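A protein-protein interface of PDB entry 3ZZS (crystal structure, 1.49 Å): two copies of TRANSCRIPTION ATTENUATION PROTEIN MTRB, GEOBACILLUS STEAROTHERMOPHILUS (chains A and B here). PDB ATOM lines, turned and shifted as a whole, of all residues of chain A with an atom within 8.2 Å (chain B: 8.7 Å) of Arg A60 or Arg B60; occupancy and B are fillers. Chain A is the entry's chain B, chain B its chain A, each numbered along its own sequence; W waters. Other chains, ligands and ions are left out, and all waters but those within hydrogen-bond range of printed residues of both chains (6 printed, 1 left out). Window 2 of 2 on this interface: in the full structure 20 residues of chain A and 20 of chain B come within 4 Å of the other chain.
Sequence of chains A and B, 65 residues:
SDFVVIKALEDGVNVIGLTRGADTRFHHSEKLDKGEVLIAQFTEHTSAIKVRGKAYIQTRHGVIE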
ATOM      1  N   SER A   1     -26.892  -7.541  15.583  1.00  0.00           N
ATOM      2  CA  SER A   1     -27.433  -7.301  16.893  1.00  0.00           C
ATOM      3  C   SER A   1     -26.422  -7.140  17.999  1.00  0.00           C
ATOM      4  O   SER A   1     -25.398  -7.809  17.907  1.00  0.00           O
ATOM      5  CB  SER A   1     -28.463  -8.351  17.281  1.00  0.00           C
ATOM      6  OG  SER A   1     -29.006  -8.064  18.554  1.00  0.00           O
ATOM      7  N   ASP A   2     -26.683  -6.343  19.037  1.00  0.00           N
ATOM      8  CA  ASP A   2     -25.736  -6.173  20.139  1.00  0.00           C
ATOM      9  C   ASP A   2     -25.536  -7.488  20.875  1.00  0.00           C
ATOM     10  O   ASP A   2     -26.416  -8.345  20.891  1.00  0.00           O
ATOM     11  CB  ASP A   2     -26.222  -5.139  21.173  1.00  0.00           C
ATOM     12  CG  ASP A   2     -25.755  -3.719  20.889  1.00  0.00           C
ATOM     13  OD1 ASP A   2     -24.526  -3.444  20.950  1.00  0.00           O
ATOM     14  OD2 ASP A   2     -26.636  -2.853  20.674  1.00  0.00           O
ATOM     15  N   PHE A   3     -24.383  -7.625  21.509  1.00  0.00           N
ATOM     16  CA  PHE A   3     -24.100  -8.765  22.370  1.00  0.00           C
ATOM     17  C   PHE A   3     -23.375  -8.303  23.621  1.00  0.00           C
ATOM     18  O   PHE A   3     -22.814  -7.205  23.667  1.00  0.00           O
ATOM     19  CB  PHE A   3     -23.251  -9.815  21.639  1.00  0.00           C
ATOM     20  CG  PHE A   3     -21.860  -9.349  21.332  1.00  0.00           C
ATOM     21  CD1 PHE A   3     -21.593  -8.608  20.189  1.00  0.00           C
ATOM     22  CD2 PHE A   3     -20.827  -9.609  22.211  1.00  0.00           C
ATOM     23  CE1 PHE A   3     -20.299  -8.154  19.926  1.00  0.00           C
ATOM     24  CE2 PHE A   3     -19.547  -9.169  21.959  1.00  0.00           C
ATOM     25  CZ  PHE A   3     -19.277  -8.443  20.814  1.00  0.00           C
ATOM     26  N   VAL A   4     -23.388  -9.169  24.623  1.00  0.00           N
ATOM     27  CA  VAL A   4     -22.695  -8.915  25.869  1.00  0.00           C
ATOM     28  C   VAL A   4     -21.715 -10.059  26.141  1.00  0.00           C
ATOM     29  O   VAL A   4     -21.940 -11.186  25.711  1.00  0.00           O
ATOM     30  CB  VAL A   4     -23.694  -8.758  27.024  1.00  0.00           C
ATOM     31  CG1 VAL A   4     -24.786  -7.755  26.653  1.00  0.00           C
ATOM     32  CG2 VAL A   4     -24.322 -10.084  27.371  1.00  0.00           C
ATOM     33  N   VAL A   5     -20.622  -9.743  26.828  1.00  0.00           N
ATOM     34  CA  VAL A   5     -19.623 -10.717  27.231  1.00  0.00           C
ATOM     35  C   VAL A   5     -19.662 -10.825  28.748  1.00  0.00           C
ATOM     36  O   VAL A   5     -19.529  -9.815  29.441  1.00  0.00           O
ATOM     37  CB  VAL A   5     -18.213 -10.293  26.799  1.00  0.00           C
ATOM     38  CG1 VAL A   5     -17.175 -11.334  27.237  1.00  0.00           C
ATOM     39  CG2 VAL A   5     -18.159 -10.046  25.285  1.00  0.00           C
ATOM     40  N   ILE A  39     -20.828 -15.380  25.656  1.00  0.00           N
ATOM     41  CA  ILE A  39     -20.976 -14.261  24.741  1.00  0.00           C
ATOM     42  C   ILE A  39     -22.373 -14.393  24.143  1.00  0.00           C
ATOM     43  O   ILE A  39     -22.631 -15.313  23.373  1.00  0.00           O
ATOM     44  CB  ILE A  39     -19.882 -14.270  23.654  1.00  0.00           C
ATOM     45  CG1 ILE A  39     -18.511 -14.613  24.265  1.00  0.00           C
ATOM     46  CG2 ILE A  39     -19.840 -12.928  22.937  1.00  0.00           C
ATOM     47  CD1 ILE A  39     -17.427 -14.813  23.232  1.00  0.00           C
ATOM     48  N   GLN A  41     -25.995 -12.714  22.451  1.00  0.00           N
ATOM     49  CA  GLN A  41     -26.707 -11.662  21.733  1.00  0.00           C
ATOM     50  C   GLN A  41     -28.070 -11.340  22.330  1.00  0.00           C
ATOM     51  O   GLN A  41     -28.688 -12.165  22.986  1.00  0.00           O
ATOM     52  CB  GLN A  41     -26.929 -12.072  20.287  1.00  0.00           C
ATOM     53  CG  GLN A  41     -25.688 -12.090  19.464  1.00  0.00           C
ATOM     54  CD  GLN A  41     -25.977 -12.447  18.032  1.00  0.00           C
ATOM     55  OE1 GLN A  41     -26.605 -13.474  17.753  1.00  0.00           O
ATOM     56  NE2 GLN A  41     -25.540 -11.602  17.107  1.00  0.00           N
ATOM     57  N   ILE A  57     -18.236  -8.077  33.105  1.00  0.00           N
ATOM     58  CA  ILE A  57     -19.126  -7.927  31.962  1.00  0.00           C
ATOM     59  C   ILE A  57     -18.630  -6.823  31.044  1.00  0.00           C
ATOM     60  O   ILE A  57     -18.252  -5.737  31.513  1.00  0.00           O
ATOM     61  CB  ILE A  57     -20.571  -7.592  32.410  1.00  0.00           C
ATOM     62  CG1 ILE A  57     -21.131  -8.715  33.287  1.00  0.00           C
ATOM     63  CG2 ILE A  57     -21.486  -7.336  31.191  1.00  0.00           C
ATOM     64  CD1 ILE A  57     -22.407  -8.365  34.005  1.00  0.00           C
ATOM     65  N   GLN A  58     -18.621  -7.113  29.743  1.00  0.00           N
ATOM     66  CA  GLN A  58     -18.357  -6.112  28.719  1.00  0.00           C
ATOM     67  C   GLN A  58     -19.577  -5.953  27.828  1.00  0.00           C
ATOM     68  O   GLN A  58     -20.164  -6.941  27.361  1.00  0.00           O
ATOM     69  CB  GLN A  58     -17.158  -6.485  27.847  1.00  0.00           C
ATOM     70  CG  GLN A  58     -15.844  -6.641  28.587  1.00  0.00           C
ATOM     71  CD  GLN A  58     -14.794  -7.327  27.748  1.00  0.00           C
ATOM     72  OE1 GLN A  58     -15.115  -8.113  26.855  1.00  0.00           O
ATOM     73  NE2 GLN A  58     -13.532  -7.061  28.047  1.00  0.00           N
ATOM     74  N   THR A  59     -19.936  -4.700  27.588  1.00  0.00           N
ATOM     75  CA  THR A  59     -20.904  -4.341  26.561  1.00  0.00           C
ATOM     76  C   THR A  59     -20.374  -3.150  25.765  1.00  0.00           C
ATOM     77  O   THR A  59     -19.311  -2.620  26.070  1.00  0.00           O
ATOM     78  CB  THR A  59     -22.286  -3.954  27.139  1.00  0.00           C
ATOM     79  OG1 THR A  59     -22.233  -2.622  27.678  1.00  0.00           O
ATOM     80  CG2 THR A  59     -22.748  -4.950  28.211  1.00  0.00           C
ATOM     81  N   ARG A  60     -21.145  -2.710  24.776  1.00  0.00           N
ATOM     82  CA  ARG A  60     -20.802  -1.537  23.988  1.00  0.00           C
ATOM     83  C   ARG A  60     -20.651  -0.279  24.852  1.00  0.00           C
ATOM     84  O   ARG A  60     -19.963   0.658  24.459  1.00  0.00           O
ATOM     85  CB  ARG A  60     -21.854  -1.300  22.894  1.00  0.00           C
ATOM     86  CG  ARG A  60     -21.378  -0.378  21.789  1.00  0.00           C
ATOM     87  CD  ARG A  60     -22.275  -0.475  20.570  1.00  0.00           C
ATOM     88  NE  ARG A  60     -23.545   0.210  20.787  1.00  0.00           N
ATOM     89  CZ  ARG A  60     -23.814   1.462  20.406  1.00  0.00           C
ATOM     90  NH1 ARG A  60     -22.905   2.203  19.770  1.00  0.00           N
ATOM     91  NH2 ARG A  60     -25.008   1.983  20.658  1.00  0.00           N
ATOM     92  N   HIS A  61     -21.287  -0.263  26.025  1.00  0.00           N
ATOM     93  CA  HIS A  61     -21.271   0.928  26.881  1.00  0.00           C
ATOM     94  C   HIS A  61     -20.175   0.876  27.943  1.00  0.00           C
ATOM     95  O   HIS A  61     -20.039   1.819  28.730  1.00  0.00           O
ATOM     96  CB  HIS A  61     -22.653   1.139  27.520  1.00  0.00           C
ATOM     97  CG  HIS A  61     -23.739   1.323  26.515  1.00  0.00           C
ATOM     98  ND1 HIS A  61     -23.542   2.007  25.339  1.00  0.00           N
ATOM     99  CD2 HIS A  61     -25.031   0.910  26.498  1.00  0.00           C
ATOM    100  CE1 HIS A  61     -24.657   1.994  24.630  1.00  0.00           C
ATOM    101  NE2 HIS A  61     -25.574   1.332  25.312  1.00  0.00           N
ATOM    102  N   GLY A  62     -19.390  -0.202  27.957  1.00  0.00           N
ATOM    103  CA  GLY A  62     -18.212  -0.292  28.814  1.00  0.00           C
ATOM    104  C   GLY A  62     -18.165  -1.575  29.619  1.00  0.00           C
ATOM    105  O   GLY A  62     -18.777  -2.578  29.252  1.00  0.00           O
ATOM    106  N   VAL A  63     -17.435  -1.518  30.726  1.00  0.00           N
ATOM    107  CA  VAL A  63     -17.213  -2.654  31.601  1.00  0.00           C
ATOM    108  C   VAL A  63     -18.029  -2.515  32.877  1.00  0.00           C
ATOM    109  O   VAL A  63     -18.153  -1.414  33.423  1.00  0.00           O
ATOM    110  CB  VAL A  63     -15.722  -2.755  31.975  1.00  0.00           C
ATOM    111  CG1 VAL A  63     -15.498  -3.748  33.141  1.00  0.00           C
ATOM    112  CG2 VAL A  63     -14.909  -3.131  30.742  1.00  0.00           C
ATOM    113  N   SER B   1     -22.337 -10.258  10.207  1.00  0.00           N
ATOM    114  CA  SER B   1     -22.554 -10.615  11.638  1.00  0.00           C
ATOM    115  C   SER B   1     -21.237 -10.543  12.400  1.00  0.00           C
ATOM    116  O   SER B   1     -20.169 -10.774  11.834  1.00  0.00           O
ATOM    117  CB  SER B   1     -23.156 -12.011  11.787  1.00  0.00           C
ATOM    118  OG  SER B   1     -23.339 -12.338  13.152  1.00  0.00           O
ATOM    119  N   ASP B   2     -21.333 -10.221  13.693  1.00  0.00           N
ATOM    120  CA  ASP B   2     -20.183 -10.175  14.595  1.00  0.00           C
ATOM    121  C   ASP B   2     -19.527 -11.543  14.682  1.00  0.00           C
ATOM    122  O   ASP B   2     -20.175 -12.570  14.458  1.00  0.00           O
ATOM    123  CB  ASP B   2     -20.600  -9.791  16.022  1.00  0.00           C
ATOM    124  CG  ASP B   2     -20.630  -8.298  16.266  1.00  0.00           C
ATOM    125  OD1 ASP B   2     -19.550  -7.648  16.233  1.00  0.00           O
ATOM    126  OD2 ASP B   2     -21.729  -7.780  16.569  1.00  0.00           O
ATOM    127  N   PHE B   3     -18.260 -11.550  15.062  1.00  0.00           N
ATOM    128  CA  PHE B   3     -17.545 -12.781  15.339  1.00  0.00           C
ATOM    129  C   PHE B   3     -16.657 -12.613  16.566  1.00  0.00           C
ATOM    130  O   PHE B   3     -16.359 -11.495  16.986  1.00  0.00           O
ATOM    131  CB  PHE B   3     -16.690 -13.216  14.135  1.00  0.00           C
ATOM    132  CG  PHE B   3     -15.551 -12.282  13.836  1.00  0.00           C
ATOM    133  CD1 PHE B   3     -15.733 -11.172  13.024  1.00  0.00           C
ATOM    134  CD2 PHE B   3     -14.300 -12.499  14.394  1.00  0.00           C
ATOM    135  CE1 PHE B   3     -14.683 -10.304  12.766  1.00  0.00           C
ATOM    136  CE2 PHE B   3     -13.247 -11.642  14.143  1.00  0.00           C
ATOM    137  CZ  PHE B   3     -13.431 -10.543  13.328  1.00  0.00           C
ATOM    138  N   VAL B   4     -16.243 -13.753  17.107  1.00  0.00           N
ATOM    139  CA  VAL B   4     -15.346 -13.783  18.243  1.00  0.00           C
ATOM    140  C   VAL B   4     -14.106 -14.592  17.876  1.00  0.00           C
ATOM    141  O   VAL B   4     -14.161 -15.498  17.047  1.00  0.00           O
ATOM    142  CB  VAL B   4     -16.047 -14.376  19.470  1.00  0.00           C
ATOM    143  CG1 VAL B   4     -17.374 -13.647  19.732  1.00  0.00           C
ATOM    144  CG2 VAL B   4     -16.286 -15.857  19.278  1.00  0.00           C
ATOM    145  N   VAL B   5     -12.979 -14.226  18.472  1.00  0.00           N
ATOM    146  CA  VAL B   5     -11.715 -14.928  18.285  1.00  0.00           C
ATOM    147  C   VAL B   5     -11.361 -15.601  19.605  1.00  0.00           C
ATOM    148  O   VAL B   5     -11.261 -14.934  20.636  1.00  0.00           O
ATOM    149  CB  VAL B   5     -10.584 -13.972  17.869  1.00  0.00           C
ATOM    150  CG1 VAL B   5      -9.270 -14.735  17.647  1.00  0.00           C
ATOM    151  CG2 VAL B   5     -10.988 -13.169  16.630  1.00  0.00           C
ATOM    152  N   PHE B  42     -21.540 -15.203  15.084  1.00  0.00           N
ATOM    153  CA  PHE B  42     -22.949 -15.371  15.375  1.00  0.00           C
ATOM    154  C   PHE B  42     -23.671 -15.561  14.045  1.00  0.00           C
ATOM    155  O   PHE B  42     -23.294 -14.971  13.043  1.00  0.00           O
ATOM    156  CB  PHE B  42     -23.489 -14.176  16.143  1.00  0.00           C
ATOM    157  CG  PHE B  42     -22.959 -14.088  17.536  1.00  0.00           C
ATOM    158  CD1 PHE B  42     -23.342 -15.034  18.484  1.00  0.00           C
ATOM    159  CD2 PHE B  42     -22.067 -13.106  17.907  1.00  0.00           C
ATOM    160  CE1 PHE B  42     -22.871 -15.001  19.753  1.00  0.00           C
ATOM    161  CE2 PHE B  42     -21.580 -13.071  19.205  1.00  0.00           C
ATOM    162  CZ  PHE B  42     -21.988 -14.023  20.122  1.00  0.00           C
ATOM    163  N   ILE B  57      -9.553 -14.355  24.485  1.00  0.00           N
ATOM    164  CA  ILE B  57     -10.695 -14.067  23.611  1.00  0.00           C
ATOM    165  C   ILE B  57     -10.691 -12.608  23.172  1.00  0.00           C
ATOM    166  O   ILE B  57     -10.446 -11.716  23.987  1.00  0.00           O
ATOM    167  CB  ILE B  57     -12.026 -14.399  24.319  1.00  0.00           C
ATOM    168  CG1 ILE B  57     -12.082 -15.876  24.725  1.00  0.00           C
ATOM    169  CG2 ILE B  57     -13.232 -14.040  23.439  1.00  0.00           C
ATOM    170  CD1 ILE B  57     -13.208 -16.206  25.674  1.00  0.00           C
ATOM    171  N   GLN B  58     -10.949 -12.376  21.882  1.00  0.00           N
ATOM    172  CA  GLN B  58     -11.179 -11.034  21.366  1.00  0.00           C
ATOM    173  C   GLN B  58     -12.581 -10.945  20.798  1.00  0.00           C
ATOM    174  O   GLN B  58     -13.018 -11.830  20.066  1.00  0.00           O
ATOM    175  CB  GLN B  58     -10.183 -10.672  20.273  1.00  0.00           C
ATOM    176  CG  GLN B  58      -8.735 -10.678  20.716  1.00  0.00           C
ATOM    177  CD  GLN B  58      -7.775 -10.648  19.552  1.00  0.00           C
ATOM    178  OE1 GLN B  58      -8.104 -11.102  18.454  1.00  0.00           O
ATOM    179  NE2 GLN B  58      -6.571 -10.137  19.788  1.00  0.00           N
ATOM    180  N   THR B  59     -13.258  -9.854  21.131  1.00  0.00           N
ATOM    181  CA  THR B  59     -14.511  -9.473  20.499  1.00  0.00           C
ATOM    182  C   THR B  59     -14.481  -7.977  20.205  1.00  0.00           C
ATOM    183  O   THR B  59     -13.529  -7.281  20.550  1.00  0.00           O
ATOM    184  CB  THR B  59     -15.752  -9.769  21.378  1.00  0.00           C
ATOM    185  OG1 THR B  59     -15.872  -8.762  22.395  1.00  0.00           O
ATOM    186  CG2 THR B  59     -15.682 -11.172  22.012  1.00  0.00           C
ATOM    187  N   ARG B  60     -15.553  -7.473  19.602  1.00  0.00           N
ATOM    188  CA  ARG B  60     -15.697  -6.045  19.352  1.00  0.00           C
ATOM    189  C   ARG B  60     -15.543  -5.215  20.639  1.00  0.00           C
ATOM    190  O   ARG B  60     -15.138  -4.050  20.588  1.00  0.00           O
ATOM    191  CB  ARG B  60     -17.056  -5.773  18.685  1.00  0.00           C
ATOM    192  CG  ARG B  60     -17.301  -4.349  18.265  1.00  0.00           C
ATOM    193  CD  ARG B  60     -18.279  -4.261  17.097  1.00  0.00           C
ATOM    194  NE  ARG B  60     -19.539  -4.973  17.328  1.00  0.00           N
ATOM    195  CZ  ARG B  60     -20.591  -4.481  17.985  1.00  0.00           C
ATOM    196  NH1 ARG B  60     -20.559  -3.263  18.520  1.00  0.00           N
ATOM    197  NH2 ARG B  60     -21.690  -5.220  18.115  1.00  0.00           N
ATOM    198  N   HIS B  61     -15.839  -5.808  21.801  1.00  0.00           N
ATOM    199  CA  HIS B  61     -15.767  -5.053  23.057  1.00  0.00           C
ATOM    200  C   HIS B  61     -14.403  -5.133  23.724  1.00  0.00           C
ATOM    201  O   HIS B  61     -14.201  -4.533  24.790  1.00  0.00           O
ATOM    202  CB  HIS B  61     -16.814  -5.539  24.048  1.00  0.00           C
ATOM    203  CG  HIS B  61     -18.194  -5.548  23.503  1.00  0.00           C
ATOM    204  ND1 HIS B  61     -18.689  -4.582  22.651  1.00  0.00           N
ATOM    205  CD2 HIS B  61     -19.211  -6.409  23.731  1.00  0.00           C
ATOM    206  CE1 HIS B  61     -19.944  -4.880  22.349  1.00  0.00           C
ATOM    207  NE2 HIS B  61     -20.279  -5.982  22.992  1.00  0.00           N
ATOM    208  N   GLY B  62     -13.479  -5.858  23.106  1.00  0.00           N
ATOM    209  CA  GLY B  62     -12.098  -5.906  23.565  1.00  0.00           C
ATOM    210  C   GLY B  62     -11.678  -7.318  23.907  1.00  0.00           C
ATOM    211  O   GLY B  62     -12.187  -8.281  23.350  1.00  0.00           O
ATOM    212  N   VAL B  63     -10.737  -7.424  24.838  1.00  0.00           N
ATOM    213  CA  VAL B  63     -10.130  -8.692  25.198  1.00  0.00           C
ATOM    214  C   VAL B  63     -10.737  -9.235  26.475  1.00  0.00           C
ATOM    215  O   VAL B  63     -10.952  -8.491  27.429  1.00  0.00           O
ATOM    216  CB  VAL B  63      -8.617  -8.525  25.419  1.00  0.00           C
ATOM    217  CG1 VAL B  63      -7.998  -9.824  25.954  1.00  0.00           C
ATOM    218  CG2 VAL B  63      -7.942  -8.093  24.131  1.00  0.00           C
HETATM  219  O   HOH W   1     -23.133  -4.448  23.673  1.00  0.00           O
HETATM  220  O   HOH W   2     -25.950 -11.864  13.982  1.00  0.00           O
HETATM  221  O   HOH W   3     -22.764  -5.254  20.614  1.00  0.00           O
HETATM  222  O   HOH W   4     -14.494  -9.460  24.563  1.00  0.00           O
HETATM  223  O   HOH W   5     -23.949  -9.992  14.673  1.00  0.00           O
HETATM  224  O   HOH W   6     -16.510  -2.201  25.754  1.00  0.00           O
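A ring nitrogen (NE2) of His B61 is in hydrogen-bond range of the backbone carbonyl oxygen of Phe A3, 2.9 Å away. O of Val B63 lies within hydrogen-bond range of NE2 of Gln A58 (3.0 Å).
The backbone carbonyl oxygen (O) of Phe B42 is in hydrogen-bond range of the side-chain hydroxyl (OG) of Ser B1 (2.6 Å). OD1 of Asp B2 lies within salt-bridge range of NE of Arg B60 (2.9 Å). The side-chain hydroxyl (OG1) of Thr B59 is in hydrogen-bond range of the backbone NH (N) of His B61. The side-chain carboxylate of Asp A2 is in salt-bridge range of the guanidinium group of Arg A60, 3.8 Å away. The backbone carbonyl oxygen (O) of Val A5 sits at hydrogen-bond distance from the backbone NH (N) of Gln A58 (2.9 Å). The side-chain hydroxyl of Thr A59 lies within hydrogen-bond range of the backbone NH of His A61.
Among the printed residues, pairs that only touch across the chains: Gln A41 with Phe B42, Arg A60 with His B61, Ile A39 with Phe B42, Phe A3 with Asp B2, Ile A39 with Val B4, Phe A3 with Arg B60, Phe A3 with Thr B59, Gln A58 with His B61, Thr A59 with His B61, Arg A60 with Arg B60, Val A5 with Thr B59 and Ser A1 with Asp B2.
Printed residues of chain B within 4 Å of Thr A59: His B61 (3.8 Å). Of chain B, only Arg B60 and His B61 come within 4 Å of Arg A60. Ser B1 touches none of the printed residues of chain A. Of the printed residues of chain A, Asp B2 touches Ser A1 (3.9 Å) and Phe A3 (3.7 Å). Of the printed residues of chain A, Phe B42 touches Ile A39 (3.6 Å) and Gln A41 (3.4 Å). Gln B58 touches none of the printed residues of chain A. The nearest printed residue of chain B that does not touch Ile A39 is Thr B59 (4.2 Å).
Hydrophobic or aromatic side chains of chain B that line the printed part of chain A: Val B4, Phe B42 and His B61. Among the printed residues, 14 pairs touch across the chains. Among the printed residues, no Asp or Glu carboxylate lies within 4 Å of a Lys or Arg side-chain nitrogen of the other chain.
Phe A3 touches Asp B2, but with the chains exchanged Asp A2 does not touch Phe B3 (10.2 Å). Phe A3 touches Thr B59, but with the chains exchanged Thr A59 does not touch Phe B3 (12.8 Å). Phe A3 touches His B61, but with the chains exchanged His A61 does not touch Phe B3 (15.2 Å). Val A5 touches Thr B59, but with the chains exchanged Thr A59 does not touch Val B5 (14.9 Å). Positions printed for both chains: 1, 2, 3, 4, 5, 57, 58, 59, 60, 61, 62 and 63.
Water W3 lies within hydrogen-bond range of the side-chain carboxylate of Asp A2 (2.5 Å), the guanidinium group of Arg B60 (2.7 Å) and the backbone NH of Phe A3 (3.0 Å). Water W4 lies within hydrogen-bond range of OG1 of Thr B59 (2.7 Å), OE1 of Gln A58 (2.7 Å) and O of Gly B62 (2.9 Å). Water W1 lies within hydrogen-bond range of O of Phe A3 (2.8 Å), N of Arg A60 (2.9 Å), OD1 of Asp A2 (3.2 Å) and NE2 of His B61 (3.3 Å). Water W2 lies within hydrogen-bond range of OG of Ser B1 and NE2 of Gln A41. Water W5 lies within hydrogen-bond range of the backbone NH (N) of Asp B2, the side-chain hydroxyl (OG) of Ser B1 and the side-chain amide nitrogen (NE2) of Gln A41. Water W6 bridges O of Thr A59 (2.8 Å) and O of His B61 (3.4 Å).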
